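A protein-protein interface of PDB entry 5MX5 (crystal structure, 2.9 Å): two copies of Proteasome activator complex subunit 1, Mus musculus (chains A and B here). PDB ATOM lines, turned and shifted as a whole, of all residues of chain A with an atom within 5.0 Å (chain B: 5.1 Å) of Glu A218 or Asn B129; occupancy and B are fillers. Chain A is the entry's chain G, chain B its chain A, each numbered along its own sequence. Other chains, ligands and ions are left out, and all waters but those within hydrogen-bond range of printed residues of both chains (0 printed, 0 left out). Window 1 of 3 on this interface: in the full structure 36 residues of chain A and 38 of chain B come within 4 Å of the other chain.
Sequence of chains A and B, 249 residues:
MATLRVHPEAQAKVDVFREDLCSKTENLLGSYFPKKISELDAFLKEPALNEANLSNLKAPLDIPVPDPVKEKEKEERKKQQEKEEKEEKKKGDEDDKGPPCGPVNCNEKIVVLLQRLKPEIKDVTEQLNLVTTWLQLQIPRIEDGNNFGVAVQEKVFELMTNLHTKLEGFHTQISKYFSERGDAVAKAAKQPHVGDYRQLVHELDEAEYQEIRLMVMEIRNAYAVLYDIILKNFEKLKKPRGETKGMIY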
ATOM      1  N   LYS A 166     -29.769   4.333  32.291  1.00  0.00           N
ATOM      2  CA  LYS A 166     -29.913   4.607  30.855  1.00  0.00           C
ATOM      3  C   LYS A 166     -31.347   4.996  30.486  1.00  0.00           C
ATOM      4  O   LYS A 166     -31.560   5.987  29.784  1.00  0.00           O
ATOM      5  CB  LYS A 166     -29.480   3.387  30.029  1.00  0.00           C
ATOM      6  CG  LYS A 166     -29.315   3.652  28.537  1.00  0.00           C
ATOM      7  CD  LYS A 166     -29.115   2.368  27.744  1.00  0.00           C
ATOM      8  CE  LYS A 166     -27.747   1.748  27.989  1.00  0.00           C
ATOM      9  NZ  LYS A 166     -27.513   0.551  27.134  1.00  0.00           N
ATOM     10  N   PHE A 170     -33.532   8.545  28.876  1.00  0.00           N
ATOM     11  CA  PHE A 170     -34.476   8.642  27.751  1.00  0.00           C
ATOM     12  C   PHE A 170     -35.716   9.458  28.118  1.00  0.00           C
ATOM     13  O   PHE A 170     -36.238  10.209  27.291  1.00  0.00           O
ATOM     14  CB  PHE A 170     -34.939   7.250  27.282  1.00  0.00           C
ATOM     15  CG  PHE A 170     -33.839   6.344  26.767  1.00  0.00           C
ATOM     16  CD1 PHE A 170     -32.557   6.816  26.452  1.00  0.00           C
ATOM     17  CD2 PHE A 170     -34.110   4.994  26.567  1.00  0.00           C
ATOM     18  CE1 PHE A 170     -31.579   5.952  25.975  1.00  0.00           C
ATOM     19  CE2 PHE A 170     -33.136   4.130  26.086  1.00  0.00           C
ATOM     20  CZ  PHE A 170     -31.869   4.608  25.792  1.00  0.00           C
ATOM     21  N   LEU A 214     -32.365   5.036  17.973  1.00  0.00           N
ATOM     22  CA  LEU A 214     -31.488   4.339  18.921  1.00  0.00           C
ATOM     23  C   LEU A 214     -32.174   4.022  20.250  1.00  0.00           C
ATOM     24  O   LEU A 214     -31.911   2.975  20.838  1.00  0.00           O
ATOM     25  CB  LEU A 214     -30.209   5.146  19.176  1.00  0.00           C
ATOM     26  CG  LEU A 214     -29.298   5.383  17.967  1.00  0.00           C
ATOM     27  CD1 LEU A 214     -28.165   6.326  18.339  1.00  0.00           C
ATOM     28  CD2 LEU A 214     -28.748   4.073  17.418  1.00  0.00           C
ATOM     29  N   MET A 215     -33.041   4.919  20.720  1.00  0.00           N
ATOM     30  CA  MET A 215     -33.829   4.671  21.939  1.00  0.00           C
ATOM     31  C   MET A 215     -34.754   3.458  21.798  1.00  0.00           C
ATOM     32  O   MET A 215     -34.921   2.702  22.751  1.00  0.00           O
ATOM     33  CB  MET A 215     -34.636   5.911  22.350  1.00  0.00           C
ATOM     34  CG  MET A 215     -33.804   6.981  23.042  1.00  0.00           C
ATOM     35  SD  MET A 215     -34.794   8.252  23.851  1.00  0.00           S
ATOM     36  CE  MET A 215     -35.315   9.240  22.452  1.00  0.00           C
ATOM     37  N   VAL A 216     -35.340   3.275  20.614  1.00  0.00           N
ATOM     38  CA  VAL A 216     -36.145   2.081  20.314  1.00  0.00           C
ATOM     39  C   VAL A 216     -35.272   0.819  20.311  1.00  0.00           C
ATOM     40  O   VAL A 216     -35.675  -0.212  20.856  1.00  0.00           O
ATOM     41  CB  VAL A 216     -36.910   2.226  18.972  1.00  0.00           C
ATOM     42  CG1 VAL A 216     -37.534   0.904  18.530  1.00  0.00           C
ATOM     43  CG2 VAL A 216     -37.993   3.288  19.094  1.00  0.00           C
ATOM     44  N   MET A 217     -34.091   0.906  19.697  1.00  0.00           N
ATOM     45  CA  MET A 217     -33.124  -0.200  19.696  1.00  0.00           C
ATOM     46  C   MET A 217     -32.663  -0.550  21.113  1.00  0.00           C
ATOM     47  O   MET A 217     -32.618  -1.725  21.474  1.00  0.00           O
ATOM     48  CB  MET A 217     -31.907   0.130  18.820  1.00  0.00           C
ATOM     49  CG  MET A 217     -32.201   0.166  17.328  1.00  0.00           C
ATOM     50  SD  MET A 217     -30.825   0.792  16.341  1.00  0.00           S
ATOM     51  CE  MET A 217     -29.590  -0.475  16.623  1.00  0.00           C
ATOM     52  N   GLU A 218     -32.340   0.473  21.905  1.00  0.00           N
ATOM     53  CA  GLU A 218     -31.882   0.291  23.292  1.00  0.00           C
ATOM     54  C   GLU A 218     -32.938  -0.339  24.210  1.00  0.00           C
ATOM     55  O   GLU A 218     -32.594  -1.119  25.100  1.00  0.00           O
ATOM     56  CB  GLU A 218     -31.412   1.625  23.890  1.00  0.00           C
ATOM     57  CG  GLU A 218     -30.136   2.188  23.273  1.00  0.00           C
ATOM     58  CD  GLU A 218     -28.869   1.682  23.939  1.00  0.00           C
ATOM     59  OE1 GLU A 218     -28.032   2.520  24.336  1.00  0.00           O
ATOM     60  OE2 GLU A 218     -28.709   0.449  24.065  1.00  0.00           O
ATOM     61  N   ILE A 219     -34.210   0.009  23.998  1.00  0.00           N
ATOM     62  CA  ILE A 219     -35.325  -0.582  24.757  1.00  0.00           C
ATOM     63  C   ILE A 219     -35.514  -2.061  24.394  1.00  0.00           C
ATOM     64  O   ILE A 219     -35.735  -2.889  25.279  1.00  0.00           O
ATOM     65  CB  ILE A 219     -36.645   0.211  24.556  1.00  0.00           C
ATOM     66  CG1 ILE A 219     -36.533   1.585  25.229  1.00  0.00           C
ATOM     67  CG2 ILE A 219     -37.845  -0.537  25.139  1.00  0.00           C
ATOM     68  CD1 ILE A 219     -37.589   2.583  24.799  1.00  0.00           C
ATOM     69  N   ARG A 220     -35.430  -2.380  23.104  1.00  0.00           N
ATOM     70  CA  ARG A 220     -35.474  -3.771  22.633  1.00  0.00           C
ATOM     71  C   ARG A 220     -34.292  -4.582  23.173  1.00  0.00           C
ATOM     72  O   ARG A 220     -34.468  -5.722  23.607  1.00  0.00           O
ATOM     73  CB  ARG A 220     -35.485  -3.812  21.102  1.00  0.00           C
ATOM     74  CG  ARG A 220     -35.580  -5.205  20.482  1.00  0.00           C
ATOM     75  CD  ARG A 220     -34.998  -5.234  19.078  1.00  0.00           C
ATOM     76  NE  ARG A 220     -33.590  -4.830  19.060  1.00  0.00           N
ATOM     77  CZ  ARG A 220     -32.878  -4.553  17.964  1.00  0.00           C
ATOM     78  NH1 ARG A 220     -33.414  -4.642  16.745  1.00  0.00           N
ATOM     79  NH2 ARG A 220     -31.603  -4.190  18.089  1.00  0.00           N
ATOM     80  N   ASN A 221     -33.099  -3.989  23.136  1.00  0.00           N
ATOM     81  CA  ASN A 221     -31.886  -4.626  23.670  1.00  0.00           C
ATOM     82  C   ASN A 221     -31.963  -4.847  25.183  1.00  0.00           C
ATOM     83  O   ASN A 221     -31.423  -5.829  25.690  1.00  0.00           O
ATOM     84  CB  ASN A 221     -30.635  -3.795  23.338  1.00  0.00           C
ATOM     85  CG  ASN A 221     -30.349  -3.713  21.845  1.00  0.00           C
ATOM     86  OD1 ASN A 221     -30.942  -4.431  21.035  1.00  0.00           O
ATOM     87  ND2 ASN A 221     -29.433  -2.827  21.474  1.00  0.00           N
ATOM     88  N   ALA A 222     -32.628  -3.935  25.893  1.00  0.00           N
ATOM     89  CA  ALA A 222     -32.843  -4.067  27.339  1.00  0.00           C
ATOM     90  C   ALA A 222     -33.703  -5.284  27.680  1.00  0.00           C
ATOM     91  O   ALA A 222     -33.354  -6.055  28.572  1.00  0.00           O
ATOM     92  CB  ALA A 222     -33.471  -2.800  27.905  1.00  0.00           C
ATOM     93  N   VAL B 124     -21.849   4.192  12.634  1.00  0.00           N
ATOM     94  CA  VAL B 124     -20.897   3.704  13.647  1.00  0.00           C
ATOM     95  C   VAL B 124     -21.526   3.470  15.030  1.00  0.00           C
ATOM     96  O   VAL B 124     -21.154   2.518  15.718  1.00  0.00           O
ATOM     97  CB  VAL B 124     -19.647   4.622  13.764  1.00  0.00           C
ATOM     98  CG1 VAL B 124     -19.992   5.978  14.374  1.00  0.00           C
ATOM     99  CG2 VAL B 124     -18.540   3.937  14.560  1.00  0.00           C
ATOM    100  N   THR B 125     -22.473   4.324  15.424  1.00  0.00           N
ATOM    101  CA  THR B 125     -23.197   4.154  16.691  1.00  0.00           C
ATOM    102  C   THR B 125     -24.154   2.961  16.653  1.00  0.00           C
ATOM    103  O   THR B 125     -24.248   2.221  17.632  1.00  0.00           O
ATOM    104  CB  THR B 125     -23.991   5.419  17.083  1.00  0.00           C
ATOM    105  OG1 THR B 125     -24.814   5.834  15.986  1.00  0.00           O
ATOM    106  CG2 THR B 125     -23.046   6.550  17.466  1.00  0.00           C
ATOM    107  N   GLU B 126     -24.859   2.785  15.533  1.00  0.00           N
ATOM    108  CA  GLU B 126     -25.778   1.648  15.357  1.00  0.00           C
ATOM    109  C   GLU B 126     -25.060   0.297  15.346  1.00  0.00           C
ATOM    110  O   GLU B 126     -25.511  -0.644  16.005  1.00  0.00           O
ATOM    111  CB  GLU B 126     -26.619   1.797  14.079  1.00  0.00           C
ATOM    112  CG  GLU B 126     -27.796   2.753  14.222  1.00  0.00           C
ATOM    113  CD  GLU B 126     -28.665   2.836  12.975  1.00  0.00           C
ATOM    114  OE1 GLU B 126     -28.802   1.823  12.253  1.00  0.00           O
ATOM    115  OE2 GLU B 126     -29.228   3.921  12.722  1.00  0.00           O
ATOM    116  N   GLN B 127     -23.956   0.205  14.602  1.00  0.00           N
ATOM    117  CA  GLN B 127     -23.172  -1.038  14.530  1.00  0.00           C
ATOM    118  C   GLN B 127     -22.440  -1.335  15.843  1.00  0.00           C
ATOM    119  O   GLN B 127     -22.270  -2.501  16.201  1.00  0.00           O
ATOM    120  CB  GLN B 127     -22.161  -1.017  13.367  1.00  0.00           C
ATOM    121  CG  GLN B 127     -22.691  -0.719  11.958  1.00  0.00           C
ATOM    122  CD  GLN B 127     -24.138  -1.127  11.706  1.00  0.00           C
ATOM    123  OE1 GLN B 127     -24.550  -2.245  12.013  1.00  0.00           O
ATOM    124  NE2 GLN B 127     -24.911  -0.215  11.125  1.00  0.00           N
ATOM    125  N   LEU B 128     -22.005  -0.289  16.547  1.00  0.00           N
ATOM    126  CA  LEU B 128     -21.447  -0.435  17.898  1.00  0.00           C
ATOM    127  C   LEU B 128     -22.505  -0.935  18.887  1.00  0.00           C
ATOM    128  O   LEU B 128     -22.217  -1.796  19.717  1.00  0.00           O
ATOM    129  CB  LEU B 128     -20.856   0.893  18.391  1.00  0.00           C
ATOM    130  CG  LEU B 128     -20.280   0.958  19.812  1.00  0.00           C
ATOM    131  CD1 LEU B 128     -19.234  -0.122  20.044  1.00  0.00           C
ATOM    132  CD2 LEU B 128     -19.690   2.335  20.067  1.00  0.00           C
ATOM    133  N   ASN B 129     -23.715  -0.387  18.789  1.00  0.00           N
ATOM    134  CA  ASN B 129     -24.843  -0.809  19.632  1.00  0.00           C
ATOM    135  C   ASN B 129     -25.265  -2.257  19.353  1.00  0.00           C
ATOM    136  O   ASN B 129     -25.659  -2.978  20.272  1.00  0.00           O
ATOM    137  CB  ASN B 129     -26.048   0.124  19.437  1.00  0.00           C
ATOM    138  CG  ASN B 129     -27.015   0.081  20.602  1.00  0.00           C
ATOM    139  OD1 ASN B 129     -28.114  -0.461  20.494  1.00  0.00           O
ATOM    140  ND2 ASN B 129     -26.604   0.654  21.729  1.00  0.00           N
ATOM    141  N   LEU B 130     -25.183  -2.665  18.086  1.00  0.00           N
ATOM    142  CA  LEU B 130     -25.498  -4.036  17.668  1.00  0.00           C
ATOM    143  C   LEU B 130     -24.465  -5.033  18.201  1.00  0.00           C
ATOM    144  O   LEU B 130     -24.830  -6.068  18.760  1.00  0.00           O
ATOM    145  CB  LEU B 130     -25.580  -4.118  16.136  1.00  0.00           C
ATOM    146  CG  LEU B 130     -26.161  -5.395  15.508  1.00  0.00           C
ATOM    147  CD1 LEU B 130     -26.951  -5.069  14.245  1.00  0.00           C
ATOM    148  CD2 LEU B 130     -25.091  -6.441  15.207  1.00  0.00           C
ATOM    149  N   VAL B 131     -23.186  -4.707  18.022  1.00  0.00           N
ATOM    150  CA  VAL B 131     -22.077  -5.565  18.465  1.00  0.00           C
ATOM    151  C   VAL B 131     -22.009  -5.665  19.999  1.00  0.00           C
ATOM    152  O   VAL B 131     -21.692  -6.729  20.536  1.00  0.00           O
ATOM    153  CB  VAL B 131     -20.721  -5.078  17.883  1.00  0.00           C
ATOM    154  CG1 VAL B 131     -19.544  -5.824  18.494  1.00  0.00           C
ATOM    155  CG2 VAL B 131     -20.696  -5.243  16.366  1.00  0.00           C
ATOM    156  N   THR B 132     -22.298  -4.562  20.690  1.00  0.00           N
ATOM    157  CA  THR B 132     -22.356  -4.545  22.158  1.00  0.00           C
ATOM    158  C   THR B 132     -23.466  -5.458  22.695  1.00  0.00           C
ATOM    159  O   THR B 132     -23.266  -6.158  23.690  1.00  0.00           O
ATOM    160  CB  THR B 132     -22.559  -3.110  22.698  1.00  0.00           C
ATOM    161  OG1 THR B 132     -21.528  -2.256  22.191  1.00  0.00           O
ATOM    162  CG2 THR B 132     -22.513  -3.078  24.221  1.00  0.00           C
ATOM    163  N   THR B 133     -24.625  -5.441  22.035  1.00  0.00           N
ATOM    164  CA  THR B 133     -25.747  -6.317  22.390  1.00  0.00           C
ATOM    165  C   THR B 133     -25.419  -7.787  22.120  1.00  0.00           C
ATOM    166  O   THR B 133     -25.749  -8.651  22.931  1.00  0.00           O
ATOM    167  CB  THR B 133     -27.027  -5.932  21.621  1.00  0.00           C
ATOM    168  OG1 THR B 133     -27.286  -4.534  21.797  1.00  0.00           O
ATOM    169  CG2 THR B 133     -28.234  -6.734  22.115  1.00  0.00           C
ATOM    170  N   HIS B 164     -18.496   4.036  22.919  1.00  0.00           N
ATOM    171  CA  HIS B 164     -19.870   4.542  23.039  1.00  0.00           C
ATOM    172  C   HIS B 164     -19.937   5.915  23.723  1.00  0.00           C
ATOM    173  O   HIS B 164     -20.747   6.760  23.339  1.00  0.00           O
ATOM    174  CB  HIS B 164     -20.743   3.530  23.792  1.00  0.00           C
ATOM    175  CG  HIS B 164     -22.185   3.922  23.886  1.00  0.00           C
ATOM    176  ND1 HIS B 164     -22.705   4.587  24.976  1.00  0.00           N
ATOM    177  CD2 HIS B 164     -23.216   3.747  23.026  1.00  0.00           C
ATOM    178  CE1 HIS B 164     -23.994   4.799  24.785  1.00  0.00           C
ATOM    179  NE2 HIS B 164     -24.329   4.301  23.609  1.00  0.00           N
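The side-chain amide nitrogen (ND2) of Asn B129 sits at hydrogen-bond distance from the side-chain carboxylate (OE2) of Glu A218, 3.2 Å away. ND2 of Asn A221 is in hydrogen-bond range of OD1 of Asn B129 (2.9 Å). The side-chain amide nitrogen of Asn A221 lies within hydrogen-bond range of the side-chain hydroxyl of Thr B133.
The backbone carbonyl oxygen (O) of Asn B129 lies within hydrogen-bond range of the side-chain hydroxyl (OG1) of Thr B133 (2.7 Å). The side-chain amino group of Lys A166 lies within salt-bridge range of the side-chain carboxylate of Glu A218 (3.3 Å). NH2 of Arg A220 sits at hydrogen-bond distance from OD1 of Asn A221, at 3.0 Å. O of Met A217 sits close to OD1 of Asn A221 (3.2 Å).
Glu B126 touches Leu A214 (CG to CD2, 3.6 Å).
Glu A218 touches one residue of chain B. Of chain A, only Glu A218 (3.2 Å) and Asn A221 (2.9 Å) come within 4 Å of Asn B129. Printed residues of chain B within 4 Å of Leu A214: Glu B126 (3.6 Å). Of the printed residues of chain A, Thr B133 touches Asn A221. The nearest residue of chain B that does not touch Glu A218 is His B164 (4.2 Å).
Of the 11 printed residues of chain B, 3 touch a printed residue of chain A. Of the 11 printed residues of chain A, 3 touch a printed residue of chain B. Hydrophobic or aromatic side chains of chain A that line the printed part of chain B: Leu A214. Among the printed residues, no Asp or Glu carboxylate lies within 4 Å of a Lys or Arg side-chain nitrogen of the other chain.
No position is printed for both chains. Of the 4 pairs that touch across the chains among the printed residues, none has its exchanged pair printed and touching as well.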
